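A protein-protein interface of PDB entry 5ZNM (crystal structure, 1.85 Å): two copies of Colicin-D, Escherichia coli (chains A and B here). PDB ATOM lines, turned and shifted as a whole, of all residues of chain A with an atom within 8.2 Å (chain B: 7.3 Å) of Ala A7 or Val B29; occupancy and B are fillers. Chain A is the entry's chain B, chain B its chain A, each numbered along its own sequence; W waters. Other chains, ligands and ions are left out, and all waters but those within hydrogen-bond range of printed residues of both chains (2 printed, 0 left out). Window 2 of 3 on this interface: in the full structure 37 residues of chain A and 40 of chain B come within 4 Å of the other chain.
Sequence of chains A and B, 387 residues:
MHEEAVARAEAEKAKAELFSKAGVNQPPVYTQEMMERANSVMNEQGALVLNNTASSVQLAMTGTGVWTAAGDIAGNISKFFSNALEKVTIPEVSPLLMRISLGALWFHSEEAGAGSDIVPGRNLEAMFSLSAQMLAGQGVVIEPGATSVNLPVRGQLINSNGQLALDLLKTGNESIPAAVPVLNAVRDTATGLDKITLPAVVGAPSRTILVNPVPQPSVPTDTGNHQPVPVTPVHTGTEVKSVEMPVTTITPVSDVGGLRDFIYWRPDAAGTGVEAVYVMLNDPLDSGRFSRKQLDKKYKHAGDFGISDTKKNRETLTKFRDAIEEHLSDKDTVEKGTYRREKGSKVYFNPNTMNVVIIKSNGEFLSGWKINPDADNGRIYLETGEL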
ATOM      1  N   HIS A   2      22.189  32.801  16.704  1.00  0.00           N
ATOM      2  CA  HIS A   2      22.493  32.780  18.126  1.00  0.00           C
ATOM      3  C   HIS A   2      21.311  33.202  18.976  1.00  0.00           C
ATOM      4  O   HIS A   2      21.508  33.683  20.107  1.00  0.00           O
ATOM      5  CB  HIS A   2      23.704  33.671  18.456  1.00  0.00           C
ATOM      6  CG  HIS A   2      24.878  33.464  17.550  1.00  0.00           C
ATOM      7  ND1 HIS A   2      25.272  32.217  17.114  1.00  0.00           N
ATOM      8  CD2 HIS A   2      25.758  34.346  17.015  1.00  0.00           C
ATOM      9  CE1 HIS A   2      26.332  32.340  16.336  1.00  0.00           C
ATOM     10  NE2 HIS A   2      26.640  33.622  16.247  1.00  0.00           N
ATOM     11  N   GLU A   3      20.092  33.061  18.440  1.00  0.00           N
ATOM     12  CA  GLU A   3      18.902  33.409  19.205  1.00  0.00           C
ATOM     13  C   GLU A   3      18.813  32.577  20.474  1.00  0.00           C
ATOM     14  O   GLU A   3      18.415  33.081  21.529  1.00  0.00           O
ATOM     15  CB  GLU A   3      17.640  33.224  18.356  1.00  0.00           C
ATOM     16  CG  GLU A   3      17.411  34.333  17.340  1.00  0.00           C
ATOM     17  CD  GLU A   3      18.336  34.243  16.128  1.00  0.00           C
ATOM     18  OE1 GLU A   3      18.985  33.186  15.943  1.00  0.00           O
ATOM     19  OE2 GLU A   3      18.403  35.231  15.360  1.00  0.00           O
ATOM     20  N   GLU A   4      19.197  31.304  20.395  1.00  0.00           N
ATOM     21  CA  GLU A   4      19.172  30.466  21.586  1.00  0.00           C
ATOM     22  C   GLU A   4      20.211  30.933  22.602  1.00  0.00           C
ATOM     23  O   GLU A   4      19.933  30.976  23.807  1.00  0.00           O
ATOM     24  CB  GLU A   4      19.400  29.008  21.195  1.00  0.00           C
ATOM     25  CG  GLU A   4      19.134  28.004  22.292  1.00  0.00           C
ATOM     26  CD  GLU A   4      19.283  26.573  21.804  1.00  0.00           C
ATOM     27  OE1 GLU A   4      19.482  26.378  20.583  1.00  0.00           O
ATOM     28  OE2 GLU A   4      19.195  25.646  22.638  1.00  0.00           O
ATOM     29  N   ALA A   5      21.410  31.295  22.132  1.00  0.00           N
ATOM     30  CA  ALA A   5      22.444  31.784  23.035  1.00  0.00           C
ATOM     31  C   ALA A   5      22.001  33.060  23.738  1.00  0.00           C
ATOM     32  O   ALA A   5      22.248  33.233  24.937  1.00  0.00           O
ATOM     33  CB  ALA A   5      23.753  32.016  22.273  1.00  0.00           C
ATOM     34  N   VAL A   6      21.294  33.946  23.029  1.00  0.00           N
ATOM     35  CA  VAL A   6      20.810  35.171  23.664  1.00  0.00           C
ATOM     36  C   VAL A   6      19.768  34.853  24.738  1.00  0.00           C
ATOM     37  O   VAL A   6      19.824  35.391  25.856  1.00  0.00           O
ATOM     38  CB  VAL A   6      20.258  36.147  22.612  1.00  0.00           C
ATOM     39  CG1 VAL A   6      19.595  37.352  23.301  1.00  0.00           C
ATOM     40  CG2 VAL A   6      21.368  36.612  21.691  1.00  0.00           C
ATOM     41  N   ALA A   7      18.798  33.985  24.418  1.00  0.00           N
ATOM     42  CA  ALA A   7      17.777  33.623  25.402  1.00  0.00           C
ATOM     43  C   ALA A   7      18.401  32.984  26.638  1.00  0.00           C
ATOM     44  O   ALA A   7      17.984  33.261  27.771  1.00  0.00           O
ATOM     45  CB  ALA A   7      16.749  32.669  24.782  1.00  0.00           C
ATOM     46  N   ARG A   8      19.388  32.109  26.437  1.00  0.00           N
ATOM     47  CA  ARG A   8      20.053  31.477  27.573  1.00  0.00           C
ATOM     48  C   ARG A   8      20.812  32.493  28.411  1.00  0.00           C
ATOM     49  O   ARG A   8      20.828  32.398  29.645  1.00  0.00           O
ATOM     50  CB  ARG A   8      21.001  30.381  27.093  1.00  0.00           C
ATOM     51  CG  ARG A   8      20.281  29.170  26.540  1.00  0.00           C
ATOM     52  CD  ARG A   8      20.993  27.879  26.879  1.00  0.00           C
ATOM     53  NE  ARG A   8      20.162  26.720  26.642  1.00  0.00           N
ATOM     54  CZ  ARG A   8      19.501  26.077  27.584  1.00  0.00           C
ATOM     55  NH1 ARG A   8      19.566  26.476  28.846  1.00  0.00           N
ATOM     56  NH2 ARG A   8      18.765  25.022  27.266  1.00  0.00           N
ATOM     57  N   ALA A   9      21.467  33.462  27.775  1.00  0.00           N
ATOM     58  CA  ALA A   9      22.194  34.450  28.568  1.00  0.00           C
ATOM     59  C   ALA A   9      21.229  35.307  29.371  1.00  0.00           C
ATOM     60  O   ALA A   9      21.496  35.637  30.533  1.00  0.00           O
ATOM     61  CB  ALA A   9      23.069  35.318  27.664  1.00  0.00           C
ATOM     62  N   GLU A  10      20.094  35.662  28.770  1.00  0.00           N
ATOM     63  CA  GLU A  10      19.086  36.439  29.481  1.00  0.00           C
ATOM     64  C   GLU A  10      18.507  35.653  30.642  1.00  0.00           C
ATOM     65  O   GLU A  10      18.278  36.218  31.724  1.00  0.00           O
ATOM     66  CB  GLU A  10      17.981  36.872  28.517  1.00  0.00           C
ATOM     67  CG  GLU A  10      18.428  37.962  27.542  1.00  0.00           C
ATOM     68  CD  GLU A  10      17.389  38.240  26.473  1.00  0.00           C
ATOM     69  OE1 GLU A  10      16.484  37.396  26.302  1.00  0.00           O
ATOM     70  OE2 GLU A  10      17.481  39.293  25.806  1.00  0.00           O
ATOM     71  N   ALA A  11      18.266  34.348  30.437  1.00  0.00           N
ATOM     72  CA  ALA A  11      17.770  33.497  31.518  1.00  0.00           C
ATOM     73  C   ALA A  11      18.779  33.423  32.653  1.00  0.00           C
ATOM     74  O   ALA A  11      18.407  33.470  33.835  1.00  0.00           O
ATOM     75  CB  ALA A  11      17.473  32.091  30.999  1.00  0.00           C
ATOM     76  N   GLU A  12      20.062  33.292  32.304  1.00  0.00           N
ATOM     77  CA  GLU A  12      21.111  33.219  33.312  1.00  0.00           C
ATOM     78  C   GLU A  12      21.210  34.514  34.096  1.00  0.00           C
ATOM     79  O   GLU A  12      21.323  34.488  35.322  1.00  0.00           O
ATOM     80  CB  GLU A  12      22.446  32.882  32.662  1.00  0.00           C
ATOM     81  CG  GLU A  12      22.496  31.453  32.151  1.00  0.00           C
ATOM     82  CD  GLU A  12      22.806  30.447  33.246  1.00  0.00           C
ATOM     83  OE1 GLU A  12      22.787  29.236  32.955  1.00  0.00           O
ATOM     84  OE2 GLU A  12      23.077  30.870  34.391  1.00  0.00           O
ATOM     85  N   LYS A  13      21.134  35.656  33.414  1.00  0.00           N
ATOM     86  CA  LYS A  13      21.128  36.932  34.127  1.00  0.00           C
ATOM     87  C   LYS A  13      19.958  37.015  35.100  1.00  0.00           C
ATOM     88  O   LYS A  13      20.129  37.389  36.266  1.00  0.00           O
ATOM     89  CB  LYS A  13      21.068  38.090  33.140  1.00  0.00           C
ATOM     90  CG  LYS A  13      20.906  39.446  33.822  1.00  0.00           C
ATOM     91  CD  LYS A  13      21.389  40.553  32.920  1.00  0.00           C
ATOM     92  CE  LYS A  13      20.605  41.825  33.180  1.00  0.00           C
ATOM     93  NZ  LYS A  13      21.437  43.037  32.960  1.00  0.00           N
ATOM     94  N   ALA A  14      18.749  36.699  34.632  1.00  0.00           N
ATOM     95  CA  ALA A  14      17.578  36.793  35.503  1.00  0.00           C
ATOM     96  C   ALA A  14      17.691  35.839  36.686  1.00  0.00           C
ATOM     97  O   ALA A  14      17.275  36.165  37.803  1.00  0.00           O
ATOM     98  CB  ALA A  14      16.303  36.503  34.709  1.00  0.00           C
ATOM     99  N   ALA A 270      11.539  24.650  37.925  1.00  0.00           N
ATOM    100  CA  ALA A 270      12.312  24.842  36.705  1.00  0.00           C
ATOM    101  C   ALA A 270      13.796  25.041  36.989  1.00  0.00           C
ATOM    102  O   ALA A 270      14.623  24.832  36.095  1.00  0.00           O
ATOM    103  CB  ALA A 270      11.772  26.048  35.940  1.00  0.00           C
ATOM    104  N   THR A 272      15.214  27.928  37.547  1.00  0.00           N
ATOM    105  CA  THR A 272      15.626  29.233  37.043  1.00  0.00           C
ATOM    106  C   THR A 272      15.032  30.400  37.819  1.00  0.00           C
ATOM    107  O   THR A 272      15.388  31.560  37.546  1.00  0.00           O
ATOM    108  CB  THR A 272      15.238  29.362  35.558  1.00  0.00           C
ATOM    109  OG1 THR A 272      13.867  28.979  35.391  1.00  0.00           O
ATOM    110  CG2 THR A 272      16.110  28.452  34.721  1.00  0.00           C
ATOM    111  N   GLN B  26      18.251  18.271  27.390  1.00  0.00           N
ATOM    112  CA  GLN B  26      17.970  19.084  28.556  1.00  0.00           C
ATOM    113  C   GLN B  26      16.859  20.085  28.224  1.00  0.00           C
ATOM    114  O   GLN B  26      16.720  20.502  27.075  1.00  0.00           O
ATOM    115  CB  GLN B  26      19.231  19.805  29.014  1.00  0.00           C
ATOM    116  CG  GLN B  26      19.586  21.015  28.214  1.00  0.00           C
ATOM    117  CD  GLN B  26      20.742  21.767  28.831  1.00  0.00           C
ATOM    118  OE1 GLN B  26      21.248  21.385  29.887  1.00  0.00           O
ATOM    119  NE2 GLN B  26      21.164  22.844  28.179  1.00  0.00           N
ATOM    120  N   PRO B  27      16.033  20.448  29.208  1.00  0.00           N
ATOM    121  CA  PRO B  27      14.960  21.402  28.939  1.00  0.00           C
ATOM    122  C   PRO B  27      15.522  22.709  28.408  1.00  0.00           C
ATOM    123  O   PRO B  27      16.618  23.135  28.805  1.00  0.00           O
ATOM    124  CB  PRO B  27      14.313  21.602  30.319  1.00  0.00           C
ATOM    125  CG  PRO B  27      14.750  20.453  31.132  1.00  0.00           C
ATOM    126  CD  PRO B  27      16.059  20.007  30.610  1.00  0.00           C
ATOM    127  N   PRO B  28      14.779  23.391  27.563  1.00  0.00           N
ATOM    128  CA  PRO B  28      15.258  24.686  27.072  1.00  0.00           C
ATOM    129  C   PRO B  28      14.875  25.807  28.022  1.00  0.00           C
ATOM    130  O   PRO B  28      14.200  25.588  29.040  1.00  0.00           O
ATOM    131  CB  PRO B  28      14.541  24.810  25.727  1.00  0.00           C
ATOM    132  CG  PRO B  28      13.164  24.181  26.023  1.00  0.00           C
ATOM    133  CD  PRO B  28      13.424  23.082  27.061  1.00  0.00           C
ATOM    134  N   VAL B  29      15.313  27.007  27.717  1.00  0.00           N
ATOM    135  CA  VAL B  29      14.708  28.200  28.285  1.00  0.00           C
ATOM    136  C   VAL B  29      13.693  28.697  27.273  1.00  0.00           C
ATOM    137  O   VAL B  29      13.789  28.430  26.070  1.00  0.00           O
ATOM    138  CB  VAL B  29      15.738  29.295  28.654  1.00  0.00           C
ATOM    139  CG1 VAL B  29      16.706  28.764  29.717  1.00  0.00           C
ATOM    140  CG2 VAL B  29      16.486  29.767  27.456  1.00  0.00           C
ATOM    141  N   TYR B  30      12.688  29.403  27.767  1.00  0.00           N
ATOM    142  CA  TYR B  30      11.515  29.722  26.974  1.00  0.00           C
ATOM    143  C   TYR B  30      11.447  31.224  26.791  1.00  0.00           C
ATOM    144  O   TYR B  30      11.379  31.975  27.770  1.00  0.00           O
ATOM    145  CB  TYR B  30      10.239  29.187  27.641  1.00  0.00           C
ATOM    146  CG  TYR B  30      10.218  27.680  27.658  1.00  0.00           C
ATOM    147  CD1 TYR B  30      10.874  26.973  28.659  1.00  0.00           C
ATOM    148  CD2 TYR B  30       9.559  26.961  26.660  1.00  0.00           C
ATOM    149  CE1 TYR B  30      10.880  25.586  28.671  1.00  0.00           C
ATOM    150  CE2 TYR B  30       9.554  25.571  26.662  1.00  0.00           C
ATOM    151  CZ  TYR B  30      10.211  24.891  27.666  1.00  0.00           C
ATOM    152  OH  TYR B  30      10.204  23.523  27.661  1.00  0.00           O
ATOM    153  N   THR B  31      11.480  31.655  25.539  1.00  0.00           N
ATOM    154  CA  THR B  31      11.017  32.991  25.251  1.00  0.00           C
ATOM    155  C   THR B  31       9.523  33.077  25.536  1.00  0.00           C
ATOM    156  O   THR B  31       8.815  32.068  25.651  1.00  0.00           O
ATOM    157  CB  THR B  31      11.315  33.365  23.801  1.00  0.00           C
ATOM    158  OG1 THR B  31      10.590  32.496  22.927  1.00  0.00           O
ATOM    159  CG2 THR B  31      12.817  33.227  23.518  1.00  0.00           C
ATOM    160  N   MET B  34       7.737  31.379  22.710  1.00  0.00           N
ATOM    161  CA  MET B  34       7.750  29.927  22.848  1.00  0.00           C
ATOM    162  C   MET B  34       6.716  29.473  23.863  1.00  0.00           C
ATOM    163  O   MET B  34       5.970  28.516  23.628  1.00  0.00           O
ATOM    164  CB  MET B  34       9.128  29.440  23.282  1.00  0.00           C
ATOM    165  CG  MET B  34      10.189  29.478  22.198  1.00  0.00           C
ATOM    166  SD  MET B  34      11.809  29.113  22.884  1.00  0.00           S
ATOM    167  CE  MET B  34      11.629  27.390  23.336  1.00  0.00           C
ATOM    168  N   ARG B 187      12.246  16.923  20.126  1.00  0.00           N
ATOM    169  CA  ARG B 187      12.124  18.290  20.608  1.00  0.00           C
ATOM    170  C   ARG B 187      11.587  19.181  19.497  1.00  0.00           C
ATOM    171  O   ARG B 187      12.149  19.231  18.398  1.00  0.00           O
ATOM    172  CB  ARG B 187      13.474  18.801  21.112  1.00  0.00           C
ATOM    173  CG  ARG B 187      13.559  20.303  21.386  1.00  0.00           C
ATOM    174  CD  ARG B 187      12.786  20.723  22.656  1.00  0.00           C
ATOM    175  NE  ARG B 187      12.965  19.816  23.793  1.00  0.00           N
ATOM    176  CZ  ARG B 187      13.915  19.922  24.724  1.00  0.00           C
ATOM    177  NH1 ARG B 187      14.831  20.888  24.661  1.00  0.00           N
ATOM    178  NH2 ARG B 187      13.959  19.049  25.723  1.00  0.00           N
ATOM    179  N   THR B 191       8.122  25.246  20.080  1.00  0.00           N
ATOM    180  CA  THR B 191       7.426  25.321  21.360  1.00  0.00           C
ATOM    181  C   THR B 191       8.311  25.041  22.558  1.00  0.00           C
ATOM    182  O   THR B 191       7.923  25.392  23.675  1.00  0.00           O
ATOM    183  CB  THR B 191       6.265  24.318  21.419  1.00  0.00           C
ATOM    184  OG1 THR B 191       6.785  22.979  21.300  1.00  0.00           O
ATOM    185  CG2 THR B 191       5.235  24.583  20.323  1.00  0.00           C
ATOM    186  N   GLY B 192       9.441  24.365  22.374  1.00  0.00           N
ATOM    187  CA  GLY B 192      10.187  23.878  23.517  1.00  0.00           C
ATOM    188  C   GLY B 192       9.574  22.678  24.208  1.00  0.00           C
ATOM    189  O   GLY B 192      10.009  22.334  25.308  1.00  0.00           O
ATOM    190  N   VAL B 214       9.841  20.734  31.486  1.00  0.00           N
ATOM    191  CA  VAL B 214      10.114  21.488  32.705  1.00  0.00           C
ATOM    192  C   VAL B 214       9.466  20.752  33.872  1.00  0.00           C
ATOM    193  O   VAL B 214       8.237  20.582  33.869  1.00  0.00           O
ATOM    194  CB  VAL B 214       9.577  22.920  32.609  1.00  0.00           C
ATOM    195  CG1 VAL B 214       9.956  23.705  33.859  1.00  0.00           C
ATOM    196  CG2 VAL B 214      10.091  23.625  31.342  1.00  0.00           C
ATOM    197  N   GLN B 227      10.635  32.463  35.831  1.00  0.00           N
ATOM    198  CA  GLN B 227      10.842  32.754  34.423  1.00  0.00           C
ATOM    199  C   GLN B 227       9.810  32.008  33.589  1.00  0.00           C
ATOM    200  O   GLN B 227       9.148  31.096  34.090  1.00  0.00           O
ATOM    201  CB  GLN B 227      12.265  32.353  34.025  1.00  0.00           C
ATOM    202  CG  GLN B 227      13.325  33.069  34.870  1.00  0.00           C
ATOM    203  CD  GLN B 227      14.664  33.183  34.154  1.00  0.00           C
ATOM    204  OE1 GLN B 227      14.718  33.550  32.984  1.00  0.00           O
ATOM    205  NE2 GLN B 227      15.742  32.868  34.855  1.00  0.00           N
ATOM    206  N   PRO B 228       9.608  32.387  32.323  1.00  0.00           N
ATOM    207  CA  PRO B 228       8.532  31.756  31.538  1.00  0.00           C
ATOM    208  C   PRO B 228       8.786  30.270  31.308  1.00  0.00           C
ATOM    209  O   PRO B 228       9.880  29.858  30.920  1.00  0.00           O
ATOM    210  CB  PRO B 228       8.542  32.543  30.221  1.00  0.00           C
ATOM    211  CG  PRO B 228       9.222  33.876  30.576  1.00  0.00           C
ATOM    212  CD  PRO B 228      10.237  33.509  31.598  1.00  0.00           C
ATOM    213  N   VAL B 229       7.758  29.465  31.566  1.00  0.00           N
ATOM    214  CA  VAL B 229       7.775  28.030  31.253  1.00  0.00           C
ATOM    215  C   VAL B 229       6.375  27.618  30.834  1.00  0.00           C
ATOM    216  O   VAL B 229       5.390  28.245  31.221  1.00  0.00           O
ATOM    217  CB  VAL B 229       8.224  27.159  32.457  1.00  0.00           C
ATOM    218  CG1 VAL B 229       9.673  27.465  32.924  1.00  0.00           C
ATOM    219  CG2 VAL B 229       7.217  27.278  33.628  1.00  0.00           C
HETATM  220  O   HOH W   1      17.004  27.018  25.217  1.00  0.00           O
HETATM  221  O   HOH W   2      11.605  29.956  36.735  1.00  0.00           O
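The side-chain amide nitrogen of Gln B227 sits at hydrogen-bond distance from the backbone carbonyl oxygen of Thr A272. O of Ala A11 lies within hydrogen-bond range of NE2 of Gln B227 (2.9 Å). NE2 of Gln B26 lies close to NH2 of Arg A8 (3.4 Å). The backbone carbonyl oxygen of Pro B27 sits at hydrogen-bond distance from the guanidinium group of Arg A8 (3.2 Å).
NH1 of Arg B187 sits at hydrogen-bond distance from O of Gln B26 (3.1 Å).
Among the printed residues, pairs that only touch across the chains: Ala A7 with Val B29, Arg A8 with Pro B28, Arg A8 with Val B29, Ala A11 with Val B29, Ala A14 with Gln B227, Ala A270 with Val B214 and Ala A270 with Val B229.
Ala A7 touches just one residue of chain B: Val B29. Val B29 touches just these residues of chain A: Ala A7, Arg A8 and Ala A11. Of the printed residues of chain B, Ala A11 touches Val B29 (3.6 Å) and Gln B227 (2.9 Å). Of the printed residues of chain A, Gln B26 touches Arg A8. Of the printed residues of chain A, Val B214 touches Ala A270. Of the printed residues of chain A, Pro B28 touches Arg A8 (3.5 Å). Of the printed residues of chain A, Val B229 touches Ala A270 (3.9 Å). Arg B187 touches none of the printed residues of chain A. Thr B191 touches none of the printed residues of chain A. The nearest printed residue of chain A that does not touch Val B214 is Thr A272 (6.7 Å).
Of the 15 printed residues of chain A, 6 touch a printed residue of chain B. Hydrophobic or aromatic side chains of chain B within 4 Å of the printed part of chain A: Val B29, Val B214 and Val B229. Among the printed residues, no Asp or Glu carboxylate lies within 4 Å of a Lys or Arg side-chain nitrogen of the other chain.
No position is printed for both chains.
Water W2 lies within hydrogen-bond range of the side-chain hydroxyl of Thr A272 and the backbone NH of Gln B227. Water W1 bridges N of Val B29 (3.0 Å) and NH2 of Arg A8 (3.4 Å).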
